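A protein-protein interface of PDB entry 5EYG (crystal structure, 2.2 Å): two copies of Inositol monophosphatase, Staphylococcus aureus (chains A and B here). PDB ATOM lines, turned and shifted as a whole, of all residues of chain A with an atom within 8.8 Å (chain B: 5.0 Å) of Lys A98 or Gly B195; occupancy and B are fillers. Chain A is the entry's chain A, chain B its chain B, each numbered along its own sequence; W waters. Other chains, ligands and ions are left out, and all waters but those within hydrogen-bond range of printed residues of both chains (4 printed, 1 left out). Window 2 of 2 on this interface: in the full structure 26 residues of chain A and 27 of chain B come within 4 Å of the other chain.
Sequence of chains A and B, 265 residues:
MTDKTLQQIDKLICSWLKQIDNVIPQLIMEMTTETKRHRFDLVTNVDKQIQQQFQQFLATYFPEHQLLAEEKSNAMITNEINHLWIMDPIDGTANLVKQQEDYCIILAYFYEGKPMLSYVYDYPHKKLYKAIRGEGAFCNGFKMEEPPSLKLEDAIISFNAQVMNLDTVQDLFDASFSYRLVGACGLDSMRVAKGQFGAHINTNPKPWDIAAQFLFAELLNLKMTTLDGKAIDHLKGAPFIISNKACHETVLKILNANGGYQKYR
The side-chain amino group of Lys B194 lies within salt-bridge range of the side-chain carboxylate of Glu A101, at 3.7 Å. O of Gln A99 sits at hydrogen-bond distance from NE2 of Gln B196 (2.9 Å). The side-chain amide nitrogen of Gln B196 is in hydrogen-bond range of the side-chain carboxylate of Glu A101 (2.7 Å). The guanidinium group of Arg B191 is in hydrogen-bond range of the side-chain amide oxygen of Gln A99. The backbone carbonyl oxygen (O) of Asp B154 sits at hydrogen-bond distance from the side-chain amino group (NZ) of Lys A98 (2.7 Å).
The backbone carbonyl oxygen of Arg B191 is in hydrogen-bond range of the backbone NH of Gln B196 (2.8 Å). O of Arg B191 is in hydrogen-bond range of N of Phe B197 (3.0 Å). NZ of Lys B194 sits at hydrogen-bond distance from OE1 of Gln B196 (2.8 Å). The backbone NH (N) of Phe B177 lies within hydrogen-bond range of the backbone carbonyl oxygen (O) of Ala B155. The side-chain amide oxygen of Asn A95 sits at hydrogen-bond distance from the side-chain amide nitrogen of Gln A99 (2.9 Å).
Lys A98 touches Ile B156 (CB to CD1, 3.6 Å). Phe B177 touches Lys A98 (CE2 to CE, 3.999 Å). Lys A98 touches Gly B195 (O to O, 3.7 Å). CA of Gln B196 touches O of Lys A98 (3.5 Å). CD1 of Ile B156 touches NE2 of Gln A99, 3.8 Å away. Gln A99 touches Phe B197 (OE1 to CE1, 3.2 Å). OE1 of Glu A101 touches CZ of Arg B191, 3.9 Å away.
Printed residues of chain B within 4 Å of Lys A98: Asp B154 (2.7 Å), Ile B156 (3.6 Å), Phe B177 (3.999 Å), Gly B195 (3.7 Å) and Gln B196 (3.5 Å). Gly B195 touches just one residue of chain A: Lys A98. Printed residues of chain B within 4 Å of Glu A101: Arg B191, Lys B194 and Gln B196. Printed residues of chain A within 4 Å of Ile B156: Lys A98 and Gln A99. Printed residues of chain B within 4 Å of Gln A99: Ile B156 (3.8 Å), Arg B191 (2.8 Å), Gln B196 (2.9 Å) and Phe B197 (3.2 Å). Met B190 touches none of the printed residues of chain A. The nearest printed residue of chain B that does not touch Lys A98 is Ala B155 (4.8 Å). The nearest residue of chain A that does not touch Gly B195 is Gln A99 (5.7 Å).
Of the 14 printed residues of chain A, 3 touch a printed residue of chain B. Of the 14 printed residues of chain B, 8 touch a printed residue of chain A. Printed residues of chain B that touch a printed residue of chain A: Asp B154, Ile B156, Phe B177, Arg B191, Lys B194, Gly B195, Gln B196 and Phe B197. Among the printed residues, Asp or Glu carboxylates within 4 Å of a Lys or Arg side-chain nitrogen of the other chain: Glu A101 with Lys B194 (3.7 Å).
No position is printed for both chains.
Water W3 bridges the backbone carbonyl oxygen of Lys A98 (2.7 Å) and the backbone carbonyl oxygen of Gly B195 (2.8 Å). Water W4 lies within hydrogen-bond range of OD1 of Asp B154 (2.8 Å) and NZ of Lys A98 (3.1 Å). Water W1 lies within hydrogen-bond range of the side-chain amide nitrogen of Gln A99 (2.8 Å) and the guanidinium group of Arg B191 (3.3 Å). Water W2 bridges O of Gln A99 (3.0 Å) and NE2 of Gln B196 (3.4 Å).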
ATOM      1  N   MET A  31     -15.027 -11.887  31.632  1.00  0.00           N
ATOM      2  CA  MET A  31     -14.451 -12.026  30.304  1.00  0.00           C
ATOM      3  C   MET A  31     -15.420 -12.693  29.336  1.00  0.00           C
ATOM      4  O   MET A  31     -15.650 -12.172  28.260  1.00  0.00           O
ATOM      5  CB  MET A  31     -13.228 -12.902  30.363  1.00  0.00           C
ATOM      6  CG  MET A  31     -12.704 -13.354  28.998  1.00  0.00           C
ATOM      7  SD  MET A  31     -11.426 -14.596  29.166  1.00  0.00           S
ATOM      8  CE  MET A  31     -12.406 -16.088  29.327  1.00  0.00           C
ATOM      9  N   THR A  32     -15.933 -13.866  29.736  1.00  0.00           N
ATOM     10  CA  THR A  32     -16.955 -14.664  29.013  1.00  0.00           C
ATOM     11  C   THR A  32     -18.273 -13.886  28.775  1.00  0.00           C
ATOM     12  O   THR A  32     -18.889 -14.027  27.736  1.00  0.00           O
ATOM     13  CB  THR A  32     -17.240 -15.970  29.814  1.00  0.00           C
ATOM     14  OG1 THR A  32     -16.280 -16.970  29.459  1.00  0.00           O
ATOM     15  CG2 THR A  32     -18.612 -16.481  29.566  1.00  0.00           C
ATOM     16  N   THR A  44      -7.273  -9.691  27.896  1.00  0.00           N
ATOM     17  CA  THR A  44      -8.510  -9.602  28.698  1.00  0.00           C
ATOM     18  C   THR A  44      -8.209  -8.874  29.983  1.00  0.00           C
ATOM     19  O   THR A  44      -7.043  -8.635  30.347  1.00  0.00           O
ATOM     20  CB  THR A  44      -9.044 -11.052  29.005  1.00  0.00           C
ATOM     21  OG1 THR A  44      -8.233 -11.696  30.007  1.00  0.00           O
ATOM     22  CG2 THR A  44      -8.905 -11.888  27.778  1.00  0.00           C
ATOM     23  N   GLY A  92      -0.691 -17.982  27.439  1.00  0.00           N
ATOM     24  CA  GLY A  92      -1.783 -18.718  26.828  1.00  0.00           C
ATOM     25  C   GLY A  92      -3.121 -17.943  26.784  1.00  0.00           C
ATOM     26  O   GLY A  92      -4.175 -18.510  27.004  1.00  0.00           O
ATOM     27  N   THR A  93      -3.064 -16.661  26.482  1.00  0.00           N
ATOM     28  CA  THR A  93      -4.247 -15.812  26.446  1.00  0.00           C
ATOM     29  C   THR A  93      -5.262 -16.344  25.406  1.00  0.00           C
ATOM     30  O   THR A  93      -6.476 -16.361  25.632  1.00  0.00           O
ATOM     31  CB  THR A  93      -3.850 -14.367  26.102  1.00  0.00           C
ATOM     32  OG1 THR A  93      -2.984 -13.844  27.120  1.00  0.00           O
ATOM     33  CG2 THR A  93      -5.037 -13.478  26.052  1.00  0.00           C
ATOM     34  N   ALA A  94      -4.750 -16.812  24.284  1.00  0.00           N
ATOM     35  CA  ALA A  94      -5.617 -17.364  23.240  1.00  0.00           C
ATOM     36  C   ALA A  94      -6.347 -18.580  23.794  1.00  0.00           C
ATOM     37  O   ALA A  94      -7.552 -18.680  23.613  1.00  0.00           O
ATOM     38  CB  ALA A  94      -4.880 -17.685  21.950  1.00  0.00           C
ATOM     39  N   ASN A  95      -5.663 -19.448  24.511  1.00  0.00           N
ATOM     40  CA  ASN A  95      -6.294 -20.616  25.116  1.00  0.00           C
ATOM     41  C   ASN A  95      -7.282 -20.183  26.206  1.00  0.00           C
ATOM     42  O   ASN A  95      -8.362 -20.768  26.323  1.00  0.00           O
ATOM     43  CB  ASN A  95      -5.203 -21.545  25.694  1.00  0.00           C
ATOM     44  CG  ASN A  95      -4.472 -22.345  24.616  1.00  0.00           C
ATOM     45  OD1 ASN A  95      -4.902 -22.401  23.454  1.00  0.00           O
ATOM     46  ND2 ASN A  95      -3.391 -23.001  25.006  1.00  0.00           N
ATOM     47  N   LEU A  96      -6.928 -19.188  27.013  1.00  0.00           N
ATOM     48  CA  LEU A  96      -7.917 -18.659  27.968  1.00  0.00           C
ATOM     49  C   LEU A  96      -9.233 -18.235  27.295  1.00  0.00           C
ATOM     50  O   LEU A  96     -10.349 -18.632  27.725  1.00  0.00           O
ATOM     51  CB  LEU A  96      -7.339 -17.527  28.851  1.00  0.00           C
ATOM     52  CG  LEU A  96      -8.296 -16.683  29.718  1.00  0.00           C
ATOM     53  CD1 LEU A  96      -8.977 -17.528  30.762  1.00  0.00           C
ATOM     54  CD2 LEU A  96      -7.596 -15.539  30.428  1.00  0.00           C
ATOM     55  N   VAL A  97      -9.101 -17.430  26.232  1.00  0.00           N
ATOM     56  CA  VAL A  97     -10.281 -16.784  25.597  1.00  0.00           C
ATOM     57  C   VAL A  97     -11.086 -17.858  24.849  1.00  0.00           C
ATOM     58  O   VAL A  97     -12.287 -17.914  24.983  1.00  0.00           O
ATOM     59  CB  VAL A  97      -9.816 -15.662  24.626  1.00  0.00           C
ATOM     60  CG1 VAL A  97     -10.947 -15.117  23.772  1.00  0.00           C
ATOM     61  CG2 VAL A  97      -9.160 -14.503  25.408  1.00  0.00           C
ATOM     62  N   LYS A  98     -10.392 -18.696  24.113  1.00  0.00           N
ATOM     63  CA  LYS A  98     -11.073 -19.670  23.225  1.00  0.00           C
ATOM     64  C   LYS A  98     -11.488 -20.928  23.972  1.00  0.00           C
ATOM     65  O   LYS A  98     -12.415 -21.582  23.534  1.00  0.00           O
ATOM     66  CB  LYS A  98     -10.205 -20.009  22.026  1.00  0.00           C
ATOM     67  CG  LYS A  98      -9.879 -18.791  21.158  1.00  0.00           C
ATOM     68  CD  LYS A  98     -11.079 -18.168  20.501  1.00  0.00           C
ATOM     69  CE  LYS A  98     -10.694 -16.908  19.702  1.00  0.00           C
ATOM     70  NZ  LYS A  98     -11.840 -16.499  18.875  1.00  0.00           N
ATOM     71  N   GLN A  99     -10.764 -21.305  25.026  1.00  0.00           N
ATOM     72  CA  GLN A  99     -10.918 -22.648  25.588  1.00  0.00           C
ATOM     73  C   GLN A  99     -11.116 -22.656  27.096  1.00  0.00           C
ATOM     74  O   GLN A  99     -11.569 -23.705  27.634  1.00  0.00           O
ATOM     75  CB  GLN A  99      -9.695 -23.504  25.333  1.00  0.00           C
ATOM     76  CG  GLN A  99      -9.155 -23.580  23.905  1.00  0.00           C
ATOM     77  CD  GLN A  99      -8.223 -24.779  23.728  1.00  0.00           C
ATOM     78  OE1 GLN A  99      -8.646 -25.925  23.851  1.00  0.00           O
ATOM     79  NE2 GLN A  99      -6.938 -24.517  23.488  1.00  0.00           N
ATOM     80  N   GLN A 100     -10.760 -21.563  27.776  1.00  0.00           N
ATOM     81  CA  GLN A 100     -10.758 -21.558  29.241  1.00  0.00           C
ATOM     82  C   GLN A 100      -9.982 -22.721  29.815  1.00  0.00           C
ATOM     83  O   GLN A 100     -10.304 -23.232  30.854  1.00  0.00           O
ATOM     84  CB  GLN A 100     -12.153 -21.448  29.861  1.00  0.00           C
ATOM     85  CG  GLN A 100     -12.857 -20.142  29.495  1.00  0.00           C
ATOM     86  CD  GLN A 100     -13.565 -20.271  28.154  1.00  0.00           C
ATOM     87  OE1 GLN A 100     -14.225 -21.322  27.841  1.00  0.00           O
ATOM     88  NE2 GLN A 100     -13.395 -19.261  27.294  1.00  0.00           N
ATOM     89  N   GLU A 101      -8.900 -23.067  29.145  1.00  0.00           N
ATOM     90  CA  GLU A 101      -8.057 -24.196  29.547  1.00  0.00           C
ATOM     91  C   GLU A 101      -6.665 -24.035  28.964  1.00  0.00           C
ATOM     92  O   GLU A 101      -6.517 -23.295  28.000  1.00  0.00           O
ATOM     93  CB  GLU A 101      -8.717 -25.514  29.038  1.00  0.00           C
ATOM     94  CG  GLU A 101      -8.177 -26.770  29.661  1.00  0.00           C
ATOM     95  CD  GLU A 101      -8.883 -28.081  29.195  1.00  0.00           C
ATOM     96  OE1 GLU A 101      -9.789 -28.066  28.324  1.00  0.00           O
ATOM     97  OE2 GLU A 101      -8.490 -29.160  29.714  1.00  0.00           O
ATOM     98  N   TYR A 103      -3.780 -22.678  30.034  1.00  0.00           N
ATOM     99  CA  TYR A 103      -3.101 -21.407  30.243  1.00  0.00           C
ATOM    100  C   TYR A 103      -2.499 -21.441  31.636  1.00  0.00           C
ATOM    101  O   TYR A 103      -2.863 -22.292  32.467  1.00  0.00           O
ATOM    102  CB  TYR A 103      -4.054 -20.194  30.011  1.00  0.00           C
ATOM    103  CG  TYR A 103      -5.228 -20.120  30.976  1.00  0.00           C
ATOM    104  CD1 TYR A 103      -5.093 -19.532  32.232  1.00  0.00           C
ATOM    105  CD2 TYR A 103      -6.433 -20.756  30.697  1.00  0.00           C
ATOM    106  CE1 TYR A 103      -6.159 -19.484  33.132  1.00  0.00           C
ATOM    107  CE2 TYR A 103      -7.502 -20.717  31.613  1.00  0.00           C
ATOM    108  CZ  TYR A 103      -7.353 -20.061  32.829  1.00  0.00           C
ATOM    109  OH  TYR A 103      -8.393 -20.029  33.749  1.00  0.00           O
ATOM    110  N   PRO B 147     -22.515 -25.465  21.766  1.00  0.00           N
ATOM    111  CA  PRO B 147     -21.463 -24.412  21.859  1.00  0.00           C
ATOM    112  C   PRO B 147     -21.883 -23.159  21.079  1.00  0.00           C
ATOM    113  O   PRO B 147     -22.697 -23.303  20.145  1.00  0.00           O
ATOM    114  CB  PRO B 147     -20.254 -25.060  21.240  1.00  0.00           C
ATOM    115  CG  PRO B 147     -20.806 -26.135  20.347  1.00  0.00           C
ATOM    116  CD  PRO B 147     -22.079 -26.624  20.983  1.00  0.00           C
ATOM    117  N   LEU B 150     -19.046 -20.779  15.866  1.00  0.00           N
ATOM    118  CA  LEU B 150     -17.657 -20.412  15.627  1.00  0.00           C
ATOM    119  C   LEU B 150     -17.386 -20.453  14.142  1.00  0.00           C
ATOM    120  O   LEU B 150     -17.345 -21.533  13.532  1.00  0.00           O
ATOM    121  CB  LEU B 150     -16.675 -21.365  16.338  1.00  0.00           C
ATOM    122  CG  LEU B 150     -16.599 -21.304  17.855  1.00  0.00           C
ATOM    123  CD1 LEU B 150     -15.735 -22.452  18.349  1.00  0.00           C
ATOM    124  CD2 LEU B 150     -16.010 -19.998  18.368  1.00  0.00           C
ATOM    125  N   ASP B 154     -12.324 -17.489  13.549  1.00  0.00           N
ATOM    126  CA  ASP B 154     -12.379 -17.245  15.038  1.00  0.00           C
ATOM    127  C   ASP B 154     -12.133 -18.506  15.840  1.00  0.00           C
ATOM    128  O   ASP B 154     -12.164 -18.494  17.084  1.00  0.00           O
ATOM    129  CB  ASP B 154     -13.772 -16.762  15.399  1.00  0.00           C
ATOM    130  CG  ASP B 154     -14.099 -15.450  14.729  1.00  0.00           C
ATOM    131  OD1 ASP B 154     -13.211 -14.560  14.800  1.00  0.00           O
ATOM    132  OD2 ASP B 154     -15.213 -15.318  14.179  1.00  0.00           O
ATOM    133  N   ALA B 155     -11.900 -19.622  15.174  1.00  0.00           N
ATOM    134  CA  ALA B 155     -11.781 -20.901  15.877  1.00  0.00           C
ATOM    135  C   ALA B 155     -10.394 -21.534  15.830  1.00  0.00           C
ATOM    136  O   ALA B 155      -9.648 -21.422  14.859  1.00  0.00           O
ATOM    137  CB  ALA B 155     -12.749 -21.901  15.227  1.00  0.00           C
ATOM    138  N   ILE B 156     -10.111 -22.272  16.888  1.00  0.00           N
ATOM    139  CA  ILE B 156      -8.889 -23.103  16.938  1.00  0.00           C
ATOM    140  C   ILE B 156      -9.234 -24.403  16.267  1.00  0.00           C
ATOM    141  O   ILE B 156     -10.324 -24.956  16.528  1.00  0.00           O
ATOM    142  CB  ILE B 156      -8.490 -23.402  18.364  1.00  0.00           C
ATOM    143  CG1 ILE B 156      -8.091 -22.115  19.048  1.00  0.00           C
ATOM    144  CG2 ILE B 156      -7.384 -24.450  18.410  1.00  0.00           C
ATOM    145  CD1 ILE B 156      -7.869 -22.288  20.536  1.00  0.00           C
ATOM    146  N   PHE B 177      -8.177 -19.458  13.467  1.00  0.00           N
ATOM    147  CA  PHE B 177      -7.627 -18.566  14.441  1.00  0.00           C
ATOM    148  C   PHE B 177      -6.300 -19.074  14.930  1.00  0.00           C
ATOM    149  O   PHE B 177      -5.345 -18.336  15.039  1.00  0.00           O
ATOM    150  CB  PHE B 177      -8.576 -18.394  15.604  1.00  0.00           C
ATOM    151  CG  PHE B 177      -8.089 -17.412  16.582  1.00  0.00           C
ATOM    152  CD1 PHE B 177      -8.323 -16.059  16.402  1.00  0.00           C
ATOM    153  CD2 PHE B 177      -7.352 -17.820  17.664  1.00  0.00           C
ATOM    154  CE1 PHE B 177      -7.847 -15.139  17.304  1.00  0.00           C
ATOM    155  CE2 PHE B 177      -6.865 -16.893  18.549  1.00  0.00           C
ATOM    156  CZ  PHE B 177      -7.116 -15.567  18.367  1.00  0.00           C
ATOM    157  N   MET B 190     -13.963 -33.922  21.999  1.00  0.00           N
ATOM    158  CA  MET B 190     -14.703 -33.303  23.105  1.00  0.00           C
ATOM    159  C   MET B 190     -14.439 -31.808  23.174  1.00  0.00           C
ATOM    160  O   MET B 190     -15.341 -31.028  23.556  1.00  0.00           O
ATOM    161  CB  MET B 190     -14.428 -33.932  24.449  1.00  0.00           C
ATOM    162  CG  MET B 190     -15.061 -35.276  24.708  1.00  0.00           C
ATOM    163  SD  MET B 190     -16.885 -35.241  24.613  1.00  0.00           S
ATOM    164  CE  MET B 190     -17.041 -35.929  22.989  1.00  0.00           C
ATOM    165  N   ARG B 191     -13.237 -31.382  22.797  1.00  0.00           N
ATOM    166  CA  ARG B 191     -12.962 -29.928  22.746  1.00  0.00           C
ATOM    167  C   ARG B 191     -13.860 -29.230  21.749  1.00  0.00           C
ATOM    168  O   ARG B 191     -14.289 -28.076  21.937  1.00  0.00           O
ATOM    169  CB  ARG B 191     -11.512 -29.710  22.396  1.00  0.00           C
ATOM    170  CG  ARG B 191     -10.589 -30.284  23.483  1.00  0.00           C
ATOM    171  CD  ARG B 191      -9.587 -29.266  24.014  1.00  0.00           C
ATOM    172  NE  ARG B 191      -8.644 -29.877  24.916  1.00  0.00           N
ATOM    173  CZ  ARG B 191      -7.552 -29.277  25.403  1.00  0.00           C
ATOM    174  NH1 ARG B 191      -7.274 -28.048  25.052  1.00  0.00           N
ATOM    175  NH2 ARG B 191      -6.697 -29.920  26.201  1.00  0.00           N
ATOM    176  N   VAL B 192     -14.230 -29.941  20.649  1.00  0.00           N
ATOM    177  CA  VAL B 192     -15.208 -29.386  19.673  1.00  0.00           C
ATOM    178  C   VAL B 192     -16.564 -29.331  20.387  1.00  0.00           C
ATOM    179  O   VAL B 192     -17.261 -28.292  20.355  1.00  0.00           O
ATOM    180  CB  VAL B 192     -15.314 -30.198  18.388  1.00  0.00           C
ATOM    181  CG1 VAL B 192     -16.375 -29.601  17.454  1.00  0.00           C
ATOM    182  CG2 VAL B 192     -13.975 -30.236  17.689  1.00  0.00           C
ATOM    183  N   ALA B 193     -16.913 -30.401  21.101  1.00  0.00           N
ATOM    184  CA  ALA B 193     -18.185 -30.476  21.785  1.00  0.00           C
ATOM    185  C   ALA B 193     -18.340 -29.375  22.843  1.00  0.00           C
ATOM    186  O   ALA B 193     -19.442 -28.887  23.027  1.00  0.00           O
ATOM    187  CB  ALA B 193     -18.368 -31.851  22.369  1.00  0.00           C
ATOM    188  N   LYS B 194     -17.215 -28.986  23.465  1.00  0.00           N
ATOM    189  CA  LYS B 194     -17.221 -27.980  24.515  1.00  0.00           C
ATOM    190  C   LYS B 194     -17.154 -26.566  23.925  1.00  0.00           C
ATOM    191  O   LYS B 194     -17.257 -25.579  24.669  1.00  0.00           O
ATOM    192  CB  LYS B 194     -16.047 -28.185  25.486  1.00  0.00           C
ATOM    193  CG  LYS B 194     -16.162 -29.370  26.442  1.00  0.00           C
ATOM    194  CD  LYS B 194     -14.941 -29.499  27.353  1.00  0.00           C
ATOM    195  CE  LYS B 194     -13.906 -30.436  26.736  1.00  0.00           C
ATOM    196  NZ  LYS B 194     -12.527 -30.279  27.291  1.00  0.00           N
ATOM    197  N   GLY B 195     -16.947 -26.451  22.614  1.00  0.00           N
ATOM    198  CA  GLY B 195     -16.769 -25.120  22.010  1.00  0.00           C
ATOM    199  C   GLY B 195     -15.355 -24.554  22.102  1.00  0.00           C
ATOM    200  O   GLY B 195     -15.144 -23.398  21.786  1.00  0.00           O
ATOM    201  N   GLN B 196     -14.396 -25.345  22.581  1.00  0.00           N
ATOM    202  CA  GLN B 196     -13.011 -24.935  22.723  1.00  0.00           C
ATOM    203  C   GLN B 196     -12.276 -24.974  21.386  1.00  0.00           C
ATOM    204  O   GLN B 196     -11.380 -24.172  21.166  1.00  0.00           O
ATOM    205  CB  GLN B 196     -12.320 -25.899  23.670  1.00  0.00           C
ATOM    206  CG  GLN B 196     -12.899 -25.870  25.077  1.00  0.00           C
ATOM    207  CD  GLN B 196     -12.267 -26.945  25.942  1.00  0.00           C
ATOM    208  OE1 GLN B 196     -12.293 -28.104  25.622  1.00  0.00           O
ATOM    209  NE2 GLN B 196     -11.643 -26.539  26.987  1.00  0.00           N
ATOM    210  N   PHE B 197     -12.584 -25.972  20.555  1.00  0.00           N
ATOM    211  CA  PHE B 197     -12.091 -26.049  19.175  1.00  0.00           C
ATOM    212  C   PHE B 197     -13.280 -25.871  18.231  1.00  0.00           C
ATOM    213  O   PHE B 197     -14.415 -26.276  18.568  1.00  0.00           O
ATOM    214  CB  PHE B 197     -11.495 -27.442  18.872  1.00  0.00           C
ATOM    215  CG  PHE B 197     -10.182 -27.777  19.578  1.00  0.00           C
ATOM    216  CD1 PHE B 197      -9.461 -26.847  20.318  1.00  0.00           C
ATOM    217  CD2 PHE B 197      -9.640 -29.083  19.457  1.00  0.00           C
ATOM    218  CE1 PHE B 197      -8.261 -27.186  20.909  1.00  0.00           C
ATOM    219  CE2 PHE B 197      -8.442 -29.437  20.057  1.00  0.00           C
ATOM    220  CZ  PHE B 197      -7.767 -28.496  20.825  1.00  0.00           C
HETATM  221  O   HOH W   1      -4.761 -26.341  23.704  1.00  0.00           O
HETATM  222  O   HOH W   2     -13.295 -25.116  29.628  1.00  0.00           O
HETATM  223  O   HOH W   3     -13.630 -21.164  21.174  1.00  0.00           O
HETATM  224  O   HOH W   4     -11.245 -14.348  16.763  1.00  0.00           O
